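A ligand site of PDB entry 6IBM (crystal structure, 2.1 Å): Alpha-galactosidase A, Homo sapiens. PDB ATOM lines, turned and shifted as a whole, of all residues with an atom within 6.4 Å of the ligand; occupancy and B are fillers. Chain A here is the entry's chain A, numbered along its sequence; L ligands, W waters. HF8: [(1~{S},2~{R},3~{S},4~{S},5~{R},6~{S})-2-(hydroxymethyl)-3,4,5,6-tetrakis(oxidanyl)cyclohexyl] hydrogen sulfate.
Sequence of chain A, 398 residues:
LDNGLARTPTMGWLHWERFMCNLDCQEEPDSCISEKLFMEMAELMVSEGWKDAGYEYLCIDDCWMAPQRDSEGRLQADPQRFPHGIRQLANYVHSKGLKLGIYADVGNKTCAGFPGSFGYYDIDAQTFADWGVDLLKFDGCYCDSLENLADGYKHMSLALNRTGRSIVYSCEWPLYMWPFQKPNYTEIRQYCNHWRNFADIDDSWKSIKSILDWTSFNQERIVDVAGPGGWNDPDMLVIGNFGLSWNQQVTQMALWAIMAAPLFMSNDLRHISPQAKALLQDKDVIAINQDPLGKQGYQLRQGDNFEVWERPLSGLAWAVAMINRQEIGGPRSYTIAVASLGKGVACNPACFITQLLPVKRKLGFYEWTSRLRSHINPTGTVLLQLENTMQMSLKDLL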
ATOM      1  N   LEU A  14      29.563  15.722  37.383  1.00  0.00           N
ATOM      2  CA  LEU A  14      28.660  15.920  36.233  1.00  0.00           C
ATOM      3  C   LEU A  14      28.025  14.558  35.882  1.00  0.00           C
ATOM      4  O   LEU A  14      28.779  13.571  35.828  1.00  0.00           O
ATOM      5  CB  LEU A  14      29.510  16.501  35.090  1.00  0.00           C
ATOM      6  CG  LEU A  14      28.776  16.900  33.820  1.00  0.00           C
ATOM      7  CD1 LEU A  14      27.663  17.894  34.117  1.00  0.00           C
ATOM      8  CD2 LEU A  14      29.761  17.472  32.823  1.00  0.00           C
ATOM      9  N   TRP A  16      26.705  13.229  33.155  1.00  0.00           N
ATOM     10  CA  TRP A  16      26.470  12.734  31.774  1.00  0.00           C
ATOM     11  C   TRP A  16      27.038  11.324  31.535  1.00  0.00           C
ATOM     12  O   TRP A  16      26.273  10.460  31.079  1.00  0.00           O
ATOM     13  CB  TRP A  16      27.026  13.680  30.724  1.00  0.00           C
ATOM     14  CG  TRP A  16      26.630  13.218  29.364  1.00  0.00           C
ATOM     15  CD1 TRP A  16      27.442  12.742  28.369  1.00  0.00           C
ATOM     16  CD2 TRP A  16      25.301  13.168  28.855  1.00  0.00           C
ATOM     17  NE1 TRP A  16      26.703  12.424  27.269  1.00  0.00           N
ATOM     18  CE2 TRP A  16      25.385  12.671  27.537  1.00  0.00           C
ATOM     19  CE3 TRP A  16      24.044  13.503  29.381  1.00  0.00           C
ATOM     20  CZ2 TRP A  16      24.251  12.490  26.744  1.00  0.00           C
ATOM     21  CZ3 TRP A  16      22.927  13.325  28.591  1.00  0.00           C
ATOM     22  CH2 TRP A  16      23.040  12.838  27.294  1.00  0.00           C
ATOM     23  N   MET A  20      23.834   9.593  31.838  1.00  0.00           N
ATOM     24  CA  MET A  20      23.367   9.792  30.440  1.00  0.00           C
ATOM     25  C   MET A  20      21.986  10.462  30.440  1.00  0.00           C
ATOM     26  O   MET A  20      21.775  11.344  31.289  1.00  0.00           O
ATOM     27  CB  MET A  20      23.317   8.453  29.689  1.00  0.00           C
ATOM     28  CG  MET A  20      24.612   7.639  29.752  1.00  0.00           C
ATOM     29  SD  MET A  20      25.300   7.315  28.109  1.00  0.00           S
ATOM     30  CE  MET A  20      25.803   8.990  27.707  1.00  0.00           C
ATOM     31  N   ASP A  61      23.713  17.835  33.601  1.00  0.00           N
ATOM     32  CA  ASP A  61      23.995  17.823  32.144  1.00  0.00           C
ATOM     33  C   ASP A  61      22.637  17.798  31.460  1.00  0.00           C
ATOM     34  O   ASP A  61      21.670  18.214  32.102  1.00  0.00           O
ATOM     35  CB  ASP A  61      24.925  16.666  31.764  1.00  0.00           C
ATOM     36  CG  ASP A  61      25.739  16.948  30.517  1.00  0.00           C
ATOM     37  OD1 ASP A  61      25.176  16.836  29.431  1.00  0.00           O
ATOM     38  OD2 ASP A  61      26.925  17.342  30.672  1.00  0.00           O
ATOM     39  N   ASP A  62      22.558  17.295  30.237  1.00  0.00           N
ATOM     40  CA  ASP A  62      21.317  17.339  29.415  1.00  0.00           C
ATOM     41  C   ASP A  62      20.239  16.459  30.074  1.00  0.00           C
ATOM     42  O   ASP A  62      20.557  15.647  30.983  1.00  0.00           O
ATOM     43  CB  ASP A  62      21.662  16.913  27.987  1.00  0.00           C
ATOM     44  CG  ASP A  62      20.695  17.389  26.919  1.00  0.00           C
ATOM     45  OD1 ASP A  62      19.595  17.883  27.278  1.00  0.00           O
ATOM     46  OD2 ASP A  62      21.034  17.234  25.737  1.00  0.00           O
ATOM     47  N   CYS A  63      18.984  16.644  29.638  1.00  0.00           N
ATOM     48  CA  CYS A  63      17.791  15.819  29.956  1.00  0.00           C
ATOM     49  C   CYS A  63      17.218  16.163  31.350  1.00  0.00           C
ATOM     50  O   CYS A  63      16.551  15.282  31.911  1.00  0.00           O
ATOM     51  CB  CYS A  63      18.101  14.337  29.814  1.00  0.00           C
ATOM     52  SG  CYS A  63      18.733  13.917  28.159  1.00  0.00           S
ATOM     53  N   TYR A 103      22.719  22.938  32.367  1.00  0.00           N
ATOM     54  CA  TYR A 103      23.055  22.659  30.947  1.00  0.00           C
ATOM     55  C   TYR A 103      22.021  23.367  30.081  1.00  0.00           C
ATOM     56  O   TYR A 103      20.850  23.411  30.487  1.00  0.00           O
ATOM     57  CB  TYR A 103      23.070  21.145  30.723  1.00  0.00           C
ATOM     58  CG  TYR A 103      23.144  20.678  29.280  1.00  0.00           C
ATOM     59  CD1 TYR A 103      22.026  20.689  28.479  1.00  0.00           C
ATOM     60  CD2 TYR A 103      24.320  20.204  28.736  1.00  0.00           C
ATOM     61  CE1 TYR A 103      22.074  20.253  27.157  1.00  0.00           C
ATOM     62  CE2 TYR A 103      24.388  19.748  27.423  1.00  0.00           C
ATOM     63  CZ  TYR A 103      23.259  19.775  26.631  1.00  0.00           C
ATOM     64  OH  TYR A 103      23.279  19.331  25.333  1.00  0.00           O
ATOM     65  N   ASP A 105      21.892  24.590  25.422  1.00  0.00           N
ATOM     66  CA  ASP A 105      22.487  24.382  24.076  1.00  0.00           C
ATOM     67  C   ASP A 105      22.332  25.689  23.275  1.00  0.00           C
ATOM     68  O   ASP A 105      21.244  26.288  23.271  1.00  0.00           O
ATOM     69  CB  ASP A 105      21.879  23.144  23.414  1.00  0.00           C
ATOM     70  CG  ASP A 105      22.563  22.722  22.120  1.00  0.00           C
ATOM     71  OD1 ASP A 105      22.518  23.512  21.135  1.00  0.00           O
ATOM     72  OD2 ASP A 105      23.149  21.616  22.097  1.00  0.00           O
ATOM     73  N   THR A 110      18.596  21.131  22.477  1.00  0.00           N
ATOM     74  CA  THR A 110      19.722  20.456  23.153  1.00  0.00           C
ATOM     75  C   THR A 110      20.087  19.217  22.332  1.00  0.00           C
ATOM     76  O   THR A 110      19.272  18.783  21.477  1.00  0.00           O
ATOM     77  CB  THR A 110      19.396  20.113  24.604  1.00  0.00           C
ATOM     78  OG1 THR A 110      18.547  18.973  24.597  1.00  0.00           O
ATOM     79  CG2 THR A 110      18.763  21.274  25.344  1.00  0.00           C
ATOM     80  N   CYS A 111      21.258  18.638  22.581  1.00  0.00           N
ATOM     81  CA  CYS A 111      21.697  17.456  21.812  1.00  0.00           C
ATOM     82  C   CYS A 111      20.700  16.317  21.961  1.00  0.00           C
ATOM     83  O   CYS A 111      20.494  15.589  20.968  1.00  0.00           O
ATOM     84  CB  CYS A 111      23.088  17.006  22.233  1.00  0.00           C
ATOM     85  SG  CYS A 111      24.306  18.294  21.883  1.00  0.00           S
ATOM     86  N   ALA A 112      20.102  16.162  23.141  1.00  0.00           N
ATOM     87  CA  ALA A 112      19.141  15.058  23.404  1.00  0.00           C
ATOM     88  C   ALA A 112      17.710  15.484  23.022  1.00  0.00           C
ATOM     89  O   ALA A 112      16.804  14.656  23.145  1.00  0.00           O
ATOM     90  CB  ALA A 112      19.258  14.617  24.848  1.00  0.00           C
ATOM     91  N   LYS A 137      27.099  24.715  31.546  1.00  0.00           N
ATOM     92  CA  LYS A 137      27.677  23.986  30.399  1.00  0.00           C
ATOM     93  C   LYS A 137      26.763  24.197  29.199  1.00  0.00           C
ATOM     94  O   LYS A 137      25.585  23.882  29.305  1.00  0.00           O
ATOM     95  CB  LYS A 137      27.829  22.497  30.736  1.00  0.00           C
ATOM     96  CG  LYS A 137      28.394  21.653  29.598  1.00  0.00           C
ATOM     97  CD  LYS A 137      28.368  20.180  29.904  1.00  0.00           C
ATOM     98  CE  LYS A 137      28.696  19.321  28.703  1.00  0.00           C
ATOM     99  NZ  LYS A 137      28.964  17.916  29.121  1.00  0.00           N
ATOM    100  N   ASP A 139      26.203  23.349  25.370  1.00  0.00           N
ATOM    101  CA  ASP A 139      26.528  22.368  24.308  1.00  0.00           C
ATOM    102  C   ASP A 139      26.177  22.990  22.937  1.00  0.00           C
ATOM    103  O   ASP A 139      25.523  24.049  22.930  1.00  0.00           O
ATOM    104  CB  ASP A 139      25.851  21.045  24.612  1.00  0.00           C
ATOM    105  CG  ASP A 139      26.550  19.821  24.077  1.00  0.00           C
ATOM    106  OD1 ASP A 139      27.380  19.941  23.181  1.00  0.00           O
ATOM    107  OD2 ASP A 139      26.158  18.546  24.642  1.00  0.00           O
ATOM    108  N   GLY A 140      26.630  22.378  21.842  1.00  0.00           N
ATOM    109  CA  GLY A 140      26.720  23.007  20.519  1.00  0.00           C
ATOM    110  C   GLY A 140      25.777  22.422  19.475  1.00  0.00           C
ATOM    111  O   GLY A 140      25.955  22.797  18.300  1.00  0.00           O
ATOM    112  N   CYS A 141      24.818  21.566  19.827  1.00  0.00           N
ATOM    113  CA  CYS A 141      23.989  20.842  18.813  1.00  0.00           C
ATOM    114  C   CYS A 141      22.947  21.767  18.172  1.00  0.00           C
ATOM    115  O   CYS A 141      22.560  22.806  18.810  1.00  0.00           O
ATOM    116  CB  CYS A 141      23.303  19.616  19.379  1.00  0.00           C
ATOM    117  SG  CYS A 141      24.453  18.274  19.810  1.00  0.00           S
ATOM    118  N   GLU A 172      31.344  24.717  24.402  1.00  0.00           N
ATOM    119  CA  GLU A 172      31.747  23.630  23.475  1.00  0.00           C
ATOM    120  C   GLU A 172      32.024  24.210  22.081  1.00  0.00           C
ATOM    121  O   GLU A 172      32.021  23.464  21.082  1.00  0.00           O
ATOM    122  CB  GLU A 172      30.724  22.497  23.513  1.00  0.00           C
ATOM    123  CG  GLU A 172      30.565  21.893  24.888  1.00  0.00           C
ATOM    124  CD  GLU A 172      30.002  20.488  24.902  1.00  0.00           C
ATOM    125  OE1 GLU A 172      29.040  20.256  25.675  1.00  0.00           O
ATOM    126  OE2 GLU A 172      30.494  19.643  24.108  1.00  0.00           O
ATOM    127  N   LEU A 175      34.985  22.520  19.885  1.00  0.00           N
ATOM    128  CA  LEU A 175      34.526  21.182  19.448  1.00  0.00           C
ATOM    129  C   LEU A 175      33.620  21.309  18.206  1.00  0.00           C
ATOM    130  O   LEU A 175      33.849  20.556  17.257  1.00  0.00           O
ATOM    131  CB  LEU A 175      33.764  20.515  20.598  1.00  0.00           C
ATOM    132  CG  LEU A 175      33.192  19.148  20.270  1.00  0.00           C
ATOM    133  CD1 LEU A 175      34.306  18.221  19.814  1.00  0.00           C
ATOM    134  CD2 LEU A 175      32.438  18.579  21.457  1.00  0.00           C
ATOM    135  N   TYR A 176      32.605  22.185  18.237  1.00  0.00           N
ATOM    136  CA  TYR A 176      31.541  22.244  17.190  1.00  0.00           C
ATOM    137  C   TYR A 176      32.002  23.024  15.954  1.00  0.00           C
ATOM    138  O   TYR A 176      31.383  22.895  14.894  1.00  0.00           O
ATOM    139  CB  TYR A 176      30.212  22.727  17.791  1.00  0.00           C
ATOM    140  CG  TYR A 176      29.541  21.593  18.514  1.00  0.00           C
ATOM    141  CD1 TYR A 176      29.836  21.338  19.843  1.00  0.00           C
ATOM    142  CD2 TYR A 176      28.719  20.688  17.852  1.00  0.00           C
ATOM    143  CE1 TYR A 176      29.282  20.267  20.516  1.00  0.00           C
ATOM    144  CE2 TYR A 176      28.144  19.605  18.522  1.00  0.00           C
ATOM    145  CZ  TYR A 176      28.440  19.394  19.859  1.00  0.00           C
ATOM    146  OH  TYR A 176      27.925  18.362  20.565  1.00  0.00           O
ATOM    147  N   ARG A 196      35.374  22.749  25.651  1.00  0.00           N
ATOM    148  CA  ARG A 196      35.527  21.383  25.132  1.00  0.00           C
ATOM    149  C   ARG A 196      36.188  21.497  23.752  1.00  0.00           C
ATOM    150  O   ARG A 196      35.688  22.233  22.901  1.00  0.00           O
ATOM    151  CB  ARG A 196      34.182  20.667  25.172  1.00  0.00           C
ATOM    152  CG  ARG A 196      33.773  20.193  26.574  1.00  0.00           C
ATOM    153  CD  ARG A 196      34.429  18.880  26.945  1.00  0.00           C
ATOM    154  NE  ARG A 196      34.258  17.941  25.850  1.00  0.00           N
ATOM    155  CZ  ARG A 196      33.122  17.284  25.577  1.00  0.00           C
ATOM    156  NH1 ARG A 196      32.066  17.397  26.369  1.00  0.00           N
ATOM    157  NH2 ARG A 196      33.065  16.514  24.487  1.00  0.00           N
ATOM    158  N   PHE A 198      37.252  18.416  22.068  1.00  0.00           N
ATOM    159  CA  PHE A 198      37.310  17.067  21.442  1.00  0.00           C
ATOM    160  C   PHE A 198      36.072  16.267  21.834  1.00  0.00           C
ATOM    161  O   PHE A 198      35.327  16.652  22.765  1.00  0.00           O
ATOM    162  CB  PHE A 198      38.634  16.393  21.834  1.00  0.00           C
ATOM    163  CG  PHE A 198      38.936  15.131  21.075  1.00  0.00           C
ATOM    164  CD1 PHE A 198      39.224  15.166  19.714  1.00  0.00           C
ATOM    165  CD2 PHE A 198      38.908  13.889  21.709  1.00  0.00           C
ATOM    166  CE1 PHE A 198      39.487  14.004  19.016  1.00  0.00           C
ATOM    167  CE2 PHE A 198      39.154  12.734  20.998  1.00  0.00           C
ATOM    168  CZ  PHE A 198      39.464  12.793  19.653  1.00  0.00           C
ATOM    169  N   ASP A 200      33.319  13.527  23.009  1.00  0.00           N
ATOM    170  CA  ASP A 200      32.898  13.032  24.345  1.00  0.00           C
ATOM    171  C   ASP A 200      33.767  11.854  24.767  1.00  0.00           C
ATOM    172  O   ASP A 200      34.032  10.959  23.934  1.00  0.00           O
ATOM    173  CB  ASP A 200      31.433  12.602  24.350  1.00  0.00           C
ATOM    174  CG  ASP A 200      30.438  13.699  23.978  1.00  0.00           C
ATOM    175  OD1 ASP A 200      30.862  14.858  23.752  1.00  0.00           O
ATOM    176  OD2 ASP A 200      29.248  13.392  23.933  1.00  0.00           O
ATOM    177  N   ASP A 235      37.260  16.810  28.907  1.00  0.00           N
ATOM    178  CA  ASP A 235      36.019  16.100  29.304  1.00  0.00           C
ATOM    179  C   ASP A 235      36.251  15.365  30.636  1.00  0.00           C
ATOM    180  O   ASP A 235      37.348  15.452  31.237  1.00  0.00           O
ATOM    181  CB  ASP A 235      35.483  15.219  28.169  1.00  0.00           C
ATOM    182  CG  ASP A 235      33.977  15.021  28.203  1.00  0.00           C
ATOM    183  OD1 ASP A 235      33.349  15.603  29.099  1.00  0.00           O
ATOM    184  OD2 ASP A 235      33.454  14.294  27.339  1.00  0.00           O
ATOM    185  N   MET A 236      35.218  14.649  31.085  1.00  0.00           N
ATOM    186  CA  MET A 236      35.025  14.162  32.476  1.00  0.00           C
ATOM    187  C   MET A 236      36.062  13.090  32.853  1.00  0.00           C
ATOM    188  O   MET A 236      36.551  12.330  31.963  1.00  0.00           O
ATOM    189  CB  MET A 236      33.620  13.577  32.582  1.00  0.00           C
ATOM    190  CG  MET A 236      32.518  14.624  32.370  1.00  0.00           C
ATOM    191  SD  MET A 236      30.898  13.841  32.118  1.00  0.00           S
ATOM    192  CE  MET A 236      30.914  13.646  30.332  1.00  0.00           C
HETATM  193  C1  HF8 L   1      28.238  16.079  25.928  1.00  0.00           C
HETATM  194  C2  HF8 L   1      26.887  15.971  26.628  1.00  0.00           C
HETATM  195  C3  HF8 L   1      25.769  15.703  25.618  1.00  0.00           C
HETATM  196  C4  HF8 L   1      26.081  16.211  24.216  1.00  0.00           C
HETATM  197  C5  HF8 L   1      26.963  17.455  24.190  1.00  0.00           C
HETATM  198  C7  HF8 L   1      28.232  17.332  25.040  1.00  0.00           C
HETATM  199  C8  HF8 L   1      24.454  16.274  26.125  1.00  0.00           C
HETATM  200  O9  HF8 L   1      23.382  15.958  25.231  1.00  0.00           O
HETATM  201  O10 HF8 L   1      26.840  15.289  23.465  1.00  0.00           O
HETATM  202  O11 HF8 L   1      26.670  17.150  27.408  1.00  0.00           O
HETATM  203  O12 HF8 L   1      29.277  16.139  26.919  1.00  0.00           O
HETATM  204  O13 HF8 L   1      29.371  17.352  24.149  1.00  0.00           O
HETATM  205  S15 HF8 L   1      26.179  14.310  22.478  1.00  0.00           S
HETATM  206  O18 HF8 L   1      27.322  13.657  21.840  1.00  0.00           O
HETATM  207  O19 HF8 L   1      25.368  13.389  23.254  1.00  0.00           O
HETATM  208  O1  HF8 L   1      25.396  15.057  21.467  1.00  0.00           O
HETATM  209  O   HOH W   1      29.323  16.070  21.653  1.00  0.00           O
HETATM  210  O   HOH W   2      30.816  13.997  27.210  1.00  0.00           O
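Water W2 bridges O12 of the ligand (2.7 Å) and OD2 of Asp 235 (2.7 Å).
Water W1 lies within hydrogen-bond range of O13 of the ligand, OD1 of Asp 200 and OH of Tyr 176.
The side-chain hydroxyl of Tyr 103 sits close to an oxygen (O9) of the ligand (3.4 Å).
The side-chain amino group (NZ) of Lys 137 is in hydrogen-bond range of an oxygen (O12) of the ligand.
OD1 of Asp 200 sits at hydrogen-bond distance from O13 of the ligand, at 2.9 Å.
The side-chain carboxylate (OD2) of Asp 139 is covalently linked to a carbon (C5) of the ligand (1.4 Å).
O12 of the ligand sits at hydrogen-bond distance from NH1 of Arg 196, at 3.1 Å.
The side-chain carboxylate (OD1) of Asp 61 lies within hydrogen-bond range of an oxygen (O11) of the ligand (2.5 Å).
The side-chain carboxylate (OD2) of Asp 62 sits at hydrogen-bond distance from an oxygen (O9) of the ligand, 2.7 Å away.
OE2 of Glu 172 is in hydrogen-bond range of O13 of the ligand (2.6 Å).
The backbone NH of Cys 141 sits at hydrogen-bond distance from the side-chain carboxylate of Asp 105 (2.8 Å).
The side-chain hydroxyl (OH) of Tyr 103 lies within hydrogen-bond range of the side-chain carboxylate (OD2) of Asp 139, 3.1 Å away.
OD2 of Asp 62 lies within hydrogen-bond range of N of Cys 111, at 3.5 Å.
The side-chain carboxylate (OD2) of Asp 62 sits at hydrogen-bond distance from the side-chain hydroxyl (OH) of Tyr 103, at 3.1 Å.
The side-chain hydroxyl of Tyr 103 sits at hydrogen-bond distance from the backbone NH of Cys 111.
The guanidinium group (NH2) of Arg 196 is in salt-bridge range of the side-chain carboxylate (OD1) of Asp 200 (2.9 Å).
The backbone NH of Leu 175 sits at hydrogen-bond distance from the backbone carbonyl oxygen of Arg 196 (3.1 Å).
N of Ala 112 lies within hydrogen-bond range of OD2 of Asp 62.
An oxygen (O1) of the ligand sits close to the side-chain sulfur (SG) of Cys 111 (3.4 Å).
The side-chain sulfur of Cys 141 sits close to an oxygen (O1) of the ligand.
Residues that only touch the ligand: Trp 16 (3.6 Å), Tyr 176 (3.9 Å) and Ala 112 (3.9 Å).
Hydrophobic or aromatic side chains within 4 Å of the ligand: Trp 16 and Tyr 103.
Within 4 Å of the ligand: Trp 16, Asp 61, Asp 62, Tyr 103, Cys 111, Ala 112, Lys 137, Asp 139, Cys 141, Glu 172, Tyr 176, Arg 196 and Asp 200.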
